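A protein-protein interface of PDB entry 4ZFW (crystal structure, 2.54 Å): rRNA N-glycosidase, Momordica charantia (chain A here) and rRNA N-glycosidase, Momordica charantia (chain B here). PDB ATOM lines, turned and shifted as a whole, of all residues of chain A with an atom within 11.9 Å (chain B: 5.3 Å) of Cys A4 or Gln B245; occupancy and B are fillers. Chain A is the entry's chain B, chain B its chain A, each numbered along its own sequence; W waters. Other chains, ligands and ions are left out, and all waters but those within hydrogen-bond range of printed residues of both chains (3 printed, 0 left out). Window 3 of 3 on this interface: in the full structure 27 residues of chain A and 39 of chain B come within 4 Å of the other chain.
The side-chain amide oxygen of Gln B202 is in hydrogen-bond range of the backbone NH of Gln B245, 2.7 Å away.
The backbone NH (N) of Cys B246 sits at hydrogen-bond distance from the side-chain amide oxygen (OE1) of Gln B202 (2.9 Å).
The backbone carbonyl oxygen (O) of Ala B203 lies within hydrogen-bond range of the side-chain hydroxyl (OG) of Ser B206 (3.2 Å).
The backbone NH (N) of Gln A3 lies close to the side-chain amide oxygen (OD1) of Asn A1 (3.4 Å).
SG of Cys B246 is disulfide-bonded to SG of Cys A4, 1.7 Å away.
O of Gln B245 sits close to SG of Cys A4 (3.5 Å).
Cys A4 touches just these residues of chain B: Ala B203, Gln B245 and Cys B246.
No residue of chain A comes within 4 Å of Thr B195.
Leu B199 touches just one residue of chain A: Gln A3 (3.9 Å).
No residue of chain A comes within 4 Å of Leu B243.
No residue of chain A comes within 4 Å of Tyr B244.
Of the printed residues of chain B, Pro A6 touches Ser B206.
Printed residues of chain B within 4 Å of Gln A3: Leu B199 (3.9 Å) and Ala B203 (3.4 Å).
Printed residues of chain A within 4 Å of Ala B203: Gln A3 (3.4 Å) and Cys A4 (3.8 Å).
Printed residues of chain B within 4 Å of Pro A51: Ser B206 (3.5 Å).
The nearest residue of chain B that does not touch Cys A4 is Leu B199 (4.1 Å).
Of the 12 printed residues of chain B, 5 touch a printed residue of chain A.
Hydrophobic or aromatic side chains of chain B that line the printed part of chain A: Leu B199 and Ala B203.
Of the 11 printed residues of chain A, 4 touch a printed residue of chain B.
Hydrophobic or aromatic side chains of chain A that line the printed part of chain B: Pro A6.
Among the printed residues, no Asp or Glu carboxylate lies within 4 Å of a Lys or Arg side-chain nitrogen of the other chain.
Water W3 lies within hydrogen-bond range of OG of Ser B206, O of Pro A6 and O of Ser A5.
Water W2 bridges O of Ser B206 (2.8 Å) and O of Pro A51 (3.2 Å).
Water W1 lies within hydrogen-bond range of the backbone carbonyl oxygen of Cys A4 (3.0 Å), the backbone carbonyl oxygen of Ala B203 (3.3 Å) and the side-chain hydroxyl of Ser B206 (3.4 Å).
CD2 of Leu B199 touches NE2 of Gln A3, at 3.9 Å.
CB of Ala B203 touches O of Gln A3, 3.4 Å away.
Cys A4 touches Ala B203.
Pro A6 touches Ser B206 (CD to OG, 3.8 Å).
CA of Pro A51 touches O of Ser B206, 3.5 Å away.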
ATOM      1  N   ASN A   1       7.563 -23.105   8.063  1.00  0.00           N
ATOM      2  CA  ASN A   1       6.118 -23.466   8.034  1.00  0.00           C
ATOM      3  C   ASN A   1       5.919 -24.865   8.638  1.00  0.00           C
ATOM      4  O   ASN A   1       6.264 -25.872   8.011  1.00  0.00           O
ATOM      5  CB  ASN A   1       5.570 -23.375   6.591  1.00  0.00           C
ATOM      6  CG  ASN A   1       4.084 -22.990   6.536  1.00  0.00           C
ATOM      7  OD1 ASN A   1       3.330 -23.236   7.480  1.00  0.00           O
ATOM      8  ND2 ASN A   1       3.661 -22.384   5.420  1.00  0.00           N
ATOM      9  N   GLU A   2       5.377 -24.903   9.845  1.00  0.00           N
ATOM     10  CA  GLU A   2       5.135 -26.140  10.543  1.00  0.00           C
ATOM     11  C   GLU A   2       3.938 -26.856   9.988  1.00  0.00           C
ATOM     12  O   GLU A   2       3.657 -27.963  10.365  1.00  0.00           O
ATOM     13  CB  GLU A   2       4.921 -25.862  12.018  1.00  0.00           C
ATOM     14  N   GLN A   3       3.214 -26.156   9.128  1.00  0.00           N
ATOM     15  CA  GLN A   3       2.060 -26.691   8.442  1.00  0.00           C
ATOM     16  C   GLN A   3       2.514 -27.632   7.348  1.00  0.00           C
ATOM     17  O   GLN A   3       1.782 -28.508   6.933  1.00  0.00           O
ATOM     18  CB  GLN A   3       1.169 -25.580   7.911  1.00  0.00           C
ATOM     19  CG  GLN A   3       0.598 -24.712   9.011  1.00  0.00           C
ATOM     20  CD  GLN A   3      -0.743 -24.118   8.654  1.00  0.00           C
ATOM     21  OE1 GLN A   3      -0.879 -22.905   8.534  1.00  0.00           O
ATOM     22  NE2 GLN A   3      -1.737 -24.973   8.464  1.00  0.00           N
ATOM     23  N   CYS A   4       3.739 -27.435   6.883  1.00  0.00           N
ATOM     24  CA  CYS A   4       4.306 -28.280   5.846  1.00  0.00           C
ATOM     25  C   CYS A   4       4.745 -29.628   6.410  1.00  0.00           C
ATOM     26  O   CYS A   4       5.051 -30.550   5.654  1.00  0.00           O
ATOM     27  CB  CYS A   4       5.488 -27.581   5.174  1.00  0.00           C
ATOM     28  SG  CYS A   4       5.076 -26.010   4.380  1.00  0.00           S
ATOM     29  N   SER A   5       4.796 -29.740   7.737  1.00  0.00           N
ATOM     30  CA  SER A   5       5.269 -30.993   8.365  1.00  0.00           C
ATOM     31  C   SER A   5       4.294 -31.482   9.420  1.00  0.00           C
ATOM     32  O   SER A   5       4.658 -31.588  10.587  1.00  0.00           O
ATOM     33  CB  SER A   5       6.654 -30.765   8.987  1.00  0.00           C
ATOM     34  OG  SER A   5       7.613 -30.454   7.996  1.00  0.00           O
ATOM     35  N   PRO A   6       3.075 -31.775   9.007  1.00  0.00           N
ATOM     36  CA  PRO A   6       2.048 -32.265   9.916  1.00  0.00           C
ATOM     37  C   PRO A   6       2.497 -33.523  10.646  1.00  0.00           C
ATOM     38  O   PRO A   6       3.038 -34.437  10.090  1.00  0.00           O
ATOM     39  CB  PRO A   6       0.861 -32.520   9.010  1.00  0.00           C
ATOM     40  CG  PRO A   6       1.425 -32.683   7.670  1.00  0.00           C
ATOM     41  CD  PRO A   6       2.669 -31.897   7.609  1.00  0.00           C
ATOM     42  N   GLN A   7       2.274 -33.515  11.933  1.00  0.00           N
ATOM     43  CA  GLN A   7       2.688 -34.590  12.786  1.00  0.00           C
ATOM     44  C   GLN A   7       1.826 -35.844  12.687  1.00  0.00           C
ATOM     45  O   GLN A   7       2.314 -36.914  12.841  1.00  0.00           O
ATOM     46  CB  GLN A   7       2.837 -34.054  14.218  1.00  0.00           C
ATOM     47  N   GLN A   8       0.549 -35.686  12.387  1.00  0.00           N
ATOM     48  CA  GLN A   8      -0.357 -36.795  12.231  1.00  0.00           C
ATOM     49  C   GLN A   8      -1.719 -36.364  11.765  1.00  0.00           C
ATOM     50  O   GLN A   8      -2.066 -35.232  11.854  1.00  0.00           O
ATOM     51  CB  GLN A   8      -0.520 -37.526  13.547  1.00  0.00           C
ATOM     52  CG  GLN A   8      -0.984 -36.640  14.670  1.00  0.00           C
ATOM     53  CD  GLN A   8      -1.374 -37.382  15.903  1.00  0.00           C
ATOM     54  OE1 GLN A   8      -0.537 -37.869  16.626  1.00  0.00           O
ATOM     55  NE2 GLN A   8      -2.643 -37.438  16.168  1.00  0.00           N
ATOM     56  N   ARG A   9      -2.487 -37.301  11.265  1.00  0.00           N
ATOM     57  CA  ARG A   9      -3.869 -37.063  10.876  1.00  0.00           C
ATOM     58  C   ARG A   9      -4.697 -38.356  11.038  1.00  0.00           C
ATOM     59  O   ARG A   9      -4.236 -39.469  10.752  1.00  0.00           O
ATOM     60  CB  ARG A   9      -3.911 -36.547   9.432  1.00  0.00           C
ATOM     61  CG  ARG A   9      -5.300 -36.171   8.934  1.00  0.00           C
ATOM     62  CD  ARG A   9      -5.716 -34.830   9.513  1.00  0.00           C
ATOM     63  NE  ARG A   9      -7.148 -34.562   9.349  1.00  0.00           N
ATOM     64  CZ  ARG A   9      -7.783 -33.543   9.924  1.00  0.00           C
ATOM     65  NH1 ARG A   9      -7.128 -32.689  10.704  1.00  0.00           N
ATOM     66  NH2 ARG A   9      -9.082 -33.384   9.728  1.00  0.00           N
ATOM     67  N   TYR A  50       1.095 -41.087  10.182  1.00  0.00           N
ATOM     68  CA  TYR A  50       2.245 -40.445  10.841  1.00  0.00           C
ATOM     69  C   TYR A  50       3.393 -40.390   9.844  1.00  0.00           C
ATOM     70  O   TYR A  50       3.336 -41.078   8.859  1.00  0.00           O
ATOM     71  CB  TYR A  50       2.692 -41.279  12.047  1.00  0.00           C
ATOM     72  CG  TYR A  50       1.724 -41.351  13.209  1.00  0.00           C
ATOM     73  CD1 TYR A  50       0.758 -42.355  13.263  1.00  0.00           C
ATOM     74  CD2 TYR A  50       1.783 -40.437  14.259  1.00  0.00           C
ATOM     75  CE1 TYR A  50      -0.131 -42.447  14.322  1.00  0.00           C
ATOM     76  CE2 TYR A  50       0.890 -40.514  15.324  1.00  0.00           C
ATOM     77  CZ  TYR A  50      -0.062 -41.534  15.361  1.00  0.00           C
ATOM     78  OH  TYR A  50      -0.969 -41.652  16.399  1.00  0.00           O
ATOM     79  N   PRO A  51       4.417 -39.605  10.117  1.00  0.00           N
ATOM     80  CA  PRO A  51       5.575 -39.479   9.234  1.00  0.00           C
ATOM     81  C   PRO A  51       6.396 -40.761   9.114  1.00  0.00           C
ATOM     82  O   PRO A  51       7.143 -40.919   8.167  1.00  0.00           O
ATOM     83  CB  PRO A  51       6.386 -38.381   9.896  1.00  0.00           C
ATOM     84  CG  PRO A  51       5.378 -37.544  10.583  1.00  0.00           C
ATOM     85  CD  PRO A  51       4.199 -38.395  10.916  1.00  0.00           C
ATOM     86  N   ILE B  38       3.170 -27.282  -9.630  1.00  0.00           N
ATOM     87  CA  ILE B  38       3.230 -26.249  -8.589  1.00  0.00           C
ATOM     88  C   ILE B  38       3.909 -25.039  -9.199  1.00  0.00           C
ATOM     89  O   ILE B  38       5.025 -25.133  -9.708  1.00  0.00           O
ATOM     90  CB  ILE B  38       4.058 -26.727  -7.368  1.00  0.00           C
ATOM     91  CG1 ILE B  38       3.418 -27.969  -6.745  1.00  0.00           C
ATOM     92  CG2 ILE B  38       4.176 -25.639  -6.292  1.00  0.00           C
ATOM     93  CD1 ILE B  38       4.362 -28.748  -5.869  1.00  0.00           C
ATOM     94  N   THR B 195      -5.488 -21.796  -2.119  1.00  0.00           N
ATOM     95  CA  THR B 195      -4.250 -21.627  -1.399  1.00  0.00           C
ATOM     96  C   THR B 195      -4.060 -22.775  -0.380  1.00  0.00           C
ATOM     97  O   THR B 195      -2.983 -23.411  -0.273  1.00  0.00           O
ATOM     98  CB  THR B 195      -4.298 -20.197  -0.803  1.00  0.00           C
ATOM     99  OG1 THR B 195      -3.486 -19.320  -1.614  1.00  0.00           O
ATOM    100  CG2 THR B 195      -3.874 -20.130   0.637  1.00  0.00           C
ATOM    101  N   SER B 198      -3.350 -26.083  -1.969  1.00  0.00           N
ATOM    102  CA  SER B 198      -1.971 -26.118  -2.399  1.00  0.00           C
ATOM    103  C   SER B 198      -1.098 -26.505  -1.236  1.00  0.00           C
ATOM    104  O   SER B 198      -0.253 -27.370  -1.350  1.00  0.00           O
ATOM    105  CB  SER B 198      -1.526 -24.769  -2.916  1.00  0.00           C
ATOM    106  OG  SER B 198      -2.273 -24.370  -4.031  1.00  0.00           O
ATOM    107  N   LEU B 199      -1.329 -25.851  -0.103  1.00  0.00           N
ATOM    108  CA  LEU B 199      -0.603 -26.162   1.130  1.00  0.00           C
ATOM    109  C   LEU B 199      -0.792 -27.592   1.567  1.00  0.00           C
ATOM    110  O   LEU B 199       0.194 -28.301   1.774  1.00  0.00           O
ATOM    111  CB  LEU B 199      -1.025 -25.231   2.257  1.00  0.00           C
ATOM    112  CG  LEU B 199      -0.419 -25.576   3.626  1.00  0.00           C
ATOM    113  CD1 LEU B 199       1.113 -25.653   3.588  1.00  0.00           C
ATOM    114  CD2 LEU B 199      -0.930 -24.550   4.628  1.00  0.00           C
ATOM    115  N   GLN B 202       0.940 -30.289  -0.711  1.00  0.00           N
ATOM    116  CA  GLN B 202       2.390 -30.326  -0.641  1.00  0.00           C
ATOM    117  C   GLN B 202       2.835 -30.873   0.688  1.00  0.00           C
ATOM    118  O   GLN B 202       3.789 -31.630   0.754  1.00  0.00           O
ATOM    119  CB  GLN B 202       2.979 -28.944  -0.926  1.00  0.00           C
ATOM    120  CG  GLN B 202       2.701 -28.536  -2.356  1.00  0.00           C
ATOM    121  CD  GLN B 202       3.012 -27.089  -2.611  1.00  0.00           C
ATOM    122  OE1 GLN B 202       4.043 -26.580  -2.185  1.00  0.00           O
ATOM    123  NE2 GLN B 202       2.121 -26.412  -3.333  1.00  0.00           N
ATOM    124  N   ALA B 203       2.123 -30.510   1.735  1.00  0.00           N
ATOM    125  CA  ALA B 203       2.359 -31.062   3.053  1.00  0.00           C
ATOM    126  C   ALA B 203       2.017 -32.544   3.115  1.00  0.00           C
ATOM    127  O   ALA B 203       2.652 -33.285   3.849  1.00  0.00           O
ATOM    128  CB  ALA B 203       1.536 -30.319   4.073  1.00  0.00           C
ATOM    129  N   SER B 206       4.612 -35.958   3.337  1.00  0.00           N
ATOM    130  CA  SER B 206       5.087 -36.604   4.543  1.00  0.00           C
ATOM    131  C   SER B 206       4.048 -37.474   5.286  1.00  0.00           C
ATOM    132  O   SER B 206       4.409 -38.071   6.308  1.00  0.00           O
ATOM    133  CB  SER B 206       5.603 -35.540   5.504  1.00  0.00           C
ATOM    134  OG  SER B 206       4.520 -34.750   5.982  1.00  0.00           O
ATOM    135  N   LEU B 243      -0.281 -23.061  -5.883  1.00  0.00           N
ATOM    136  CA  LEU B 243       0.648 -22.146  -5.274  1.00  0.00           C
ATOM    137  C   LEU B 243       1.776 -22.900  -4.549  1.00  0.00           C
ATOM    138  O   LEU B 243       1.511 -23.869  -3.821  1.00  0.00           O
ATOM    139  CB  LEU B 243      -0.100 -21.290  -4.254  1.00  0.00           C
ATOM    140  CG  LEU B 243       0.633 -20.086  -3.646  1.00  0.00           C
ATOM    141  CD1 LEU B 243       0.946 -19.076  -4.724  1.00  0.00           C
ATOM    142  CD2 LEU B 243      -0.175 -19.401  -2.552  1.00  0.00           C
ATOM    143  N   TYR B 244       3.018 -22.458  -4.748  1.00  0.00           N
ATOM    144  CA  TYR B 244       4.151 -23.046  -4.066  1.00  0.00           C
ATOM    145  C   TYR B 244       3.972 -22.805  -2.582  1.00  0.00           C
ATOM    146  O   TYR B 244       3.694 -21.679  -2.155  1.00  0.00           O
ATOM    147  CB  TYR B 244       5.480 -22.453  -4.562  1.00  0.00           C
ATOM    148  CG  TYR B 244       6.658 -22.781  -3.654  1.00  0.00           C
ATOM    149  CD1 TYR B 244       7.322 -24.000  -3.740  1.00  0.00           C
ATOM    150  CD2 TYR B 244       7.079 -21.872  -2.679  1.00  0.00           C
ATOM    151  CE1 TYR B 244       8.377 -24.298  -2.891  1.00  0.00           C
ATOM    152  CE2 TYR B 244       8.121 -22.171  -1.820  1.00  0.00           C
ATOM    153  CZ  TYR B 244       8.780 -23.375  -1.941  1.00  0.00           C
ATOM    154  OH  TYR B 244       9.825 -23.646  -1.082  1.00  0.00           O
ATOM    155  N   GLN B 245       4.089 -23.865  -1.788  1.00  0.00           N
ATOM    156  CA  GLN B 245       3.922 -23.738  -0.331  1.00  0.00           C
ATOM    157  C   GLN B 245       5.004 -24.392   0.496  1.00  0.00           C
ATOM    158  O   GLN B 245       5.298 -23.911   1.556  1.00  0.00           O
ATOM    159  CB  GLN B 245       2.577 -24.267   0.126  1.00  0.00           C
ATOM    160  CG  GLN B 245       1.376 -23.476  -0.329  1.00  0.00           C
ATOM    161  CD  GLN B 245       1.174 -22.195   0.433  1.00  0.00           C
ATOM    162  OE1 GLN B 245       1.998 -21.301   0.362  1.00  0.00           O
ATOM    163  NE2 GLN B 245       0.040 -22.067   1.090  1.00  0.00           N
ATOM    164  N   CYS B 246       5.502 -25.542   0.079  1.00  0.00           N
ATOM    165  CA  CYS B 246       6.485 -26.181   0.922  1.00  0.00           C
ATOM    166  C   CYS B 246       7.693 -26.762   0.232  1.00  0.00           C
ATOM    167  O   CYS B 246       7.583 -27.478  -0.763  1.00  0.00           O
ATOM    168  CB  CYS B 246       5.816 -27.267   1.773  1.00  0.00           C
ATOM    169  SG  CYS B 246       4.507 -26.660   2.862  1.00  0.00           S
ATOM    170  N   PRO B 247       8.852 -26.464   0.796  1.00  0.00           N
ATOM    171  CA  PRO B 247      10.096 -27.043   0.294  1.00  0.00           C
ATOM    172  C   PRO B 247      10.064 -28.546   0.338  1.00  0.00           C
ATOM    173  O   PRO B 247      10.142 -29.147  -0.721  1.00  0.00           O
ATOM    174  CB  PRO B 247      11.139 -26.519   1.263  1.00  0.00           C
ATOM    175  CG  PRO B 247      10.382 -26.218   2.504  1.00  0.00           C
ATOM    176  CD  PRO B 247       9.072 -25.707   2.047  1.00  0.00           C
HETATM  177  O   HOH W   1       5.870 -32.622   3.628  1.00  0.00           O
HETATM  178  O   HOH W   2       7.172 -38.599   5.989  1.00  0.00           O
HETATM  179  O   HOH W   3       5.304 -34.293   8.560  1.00  0.00           O
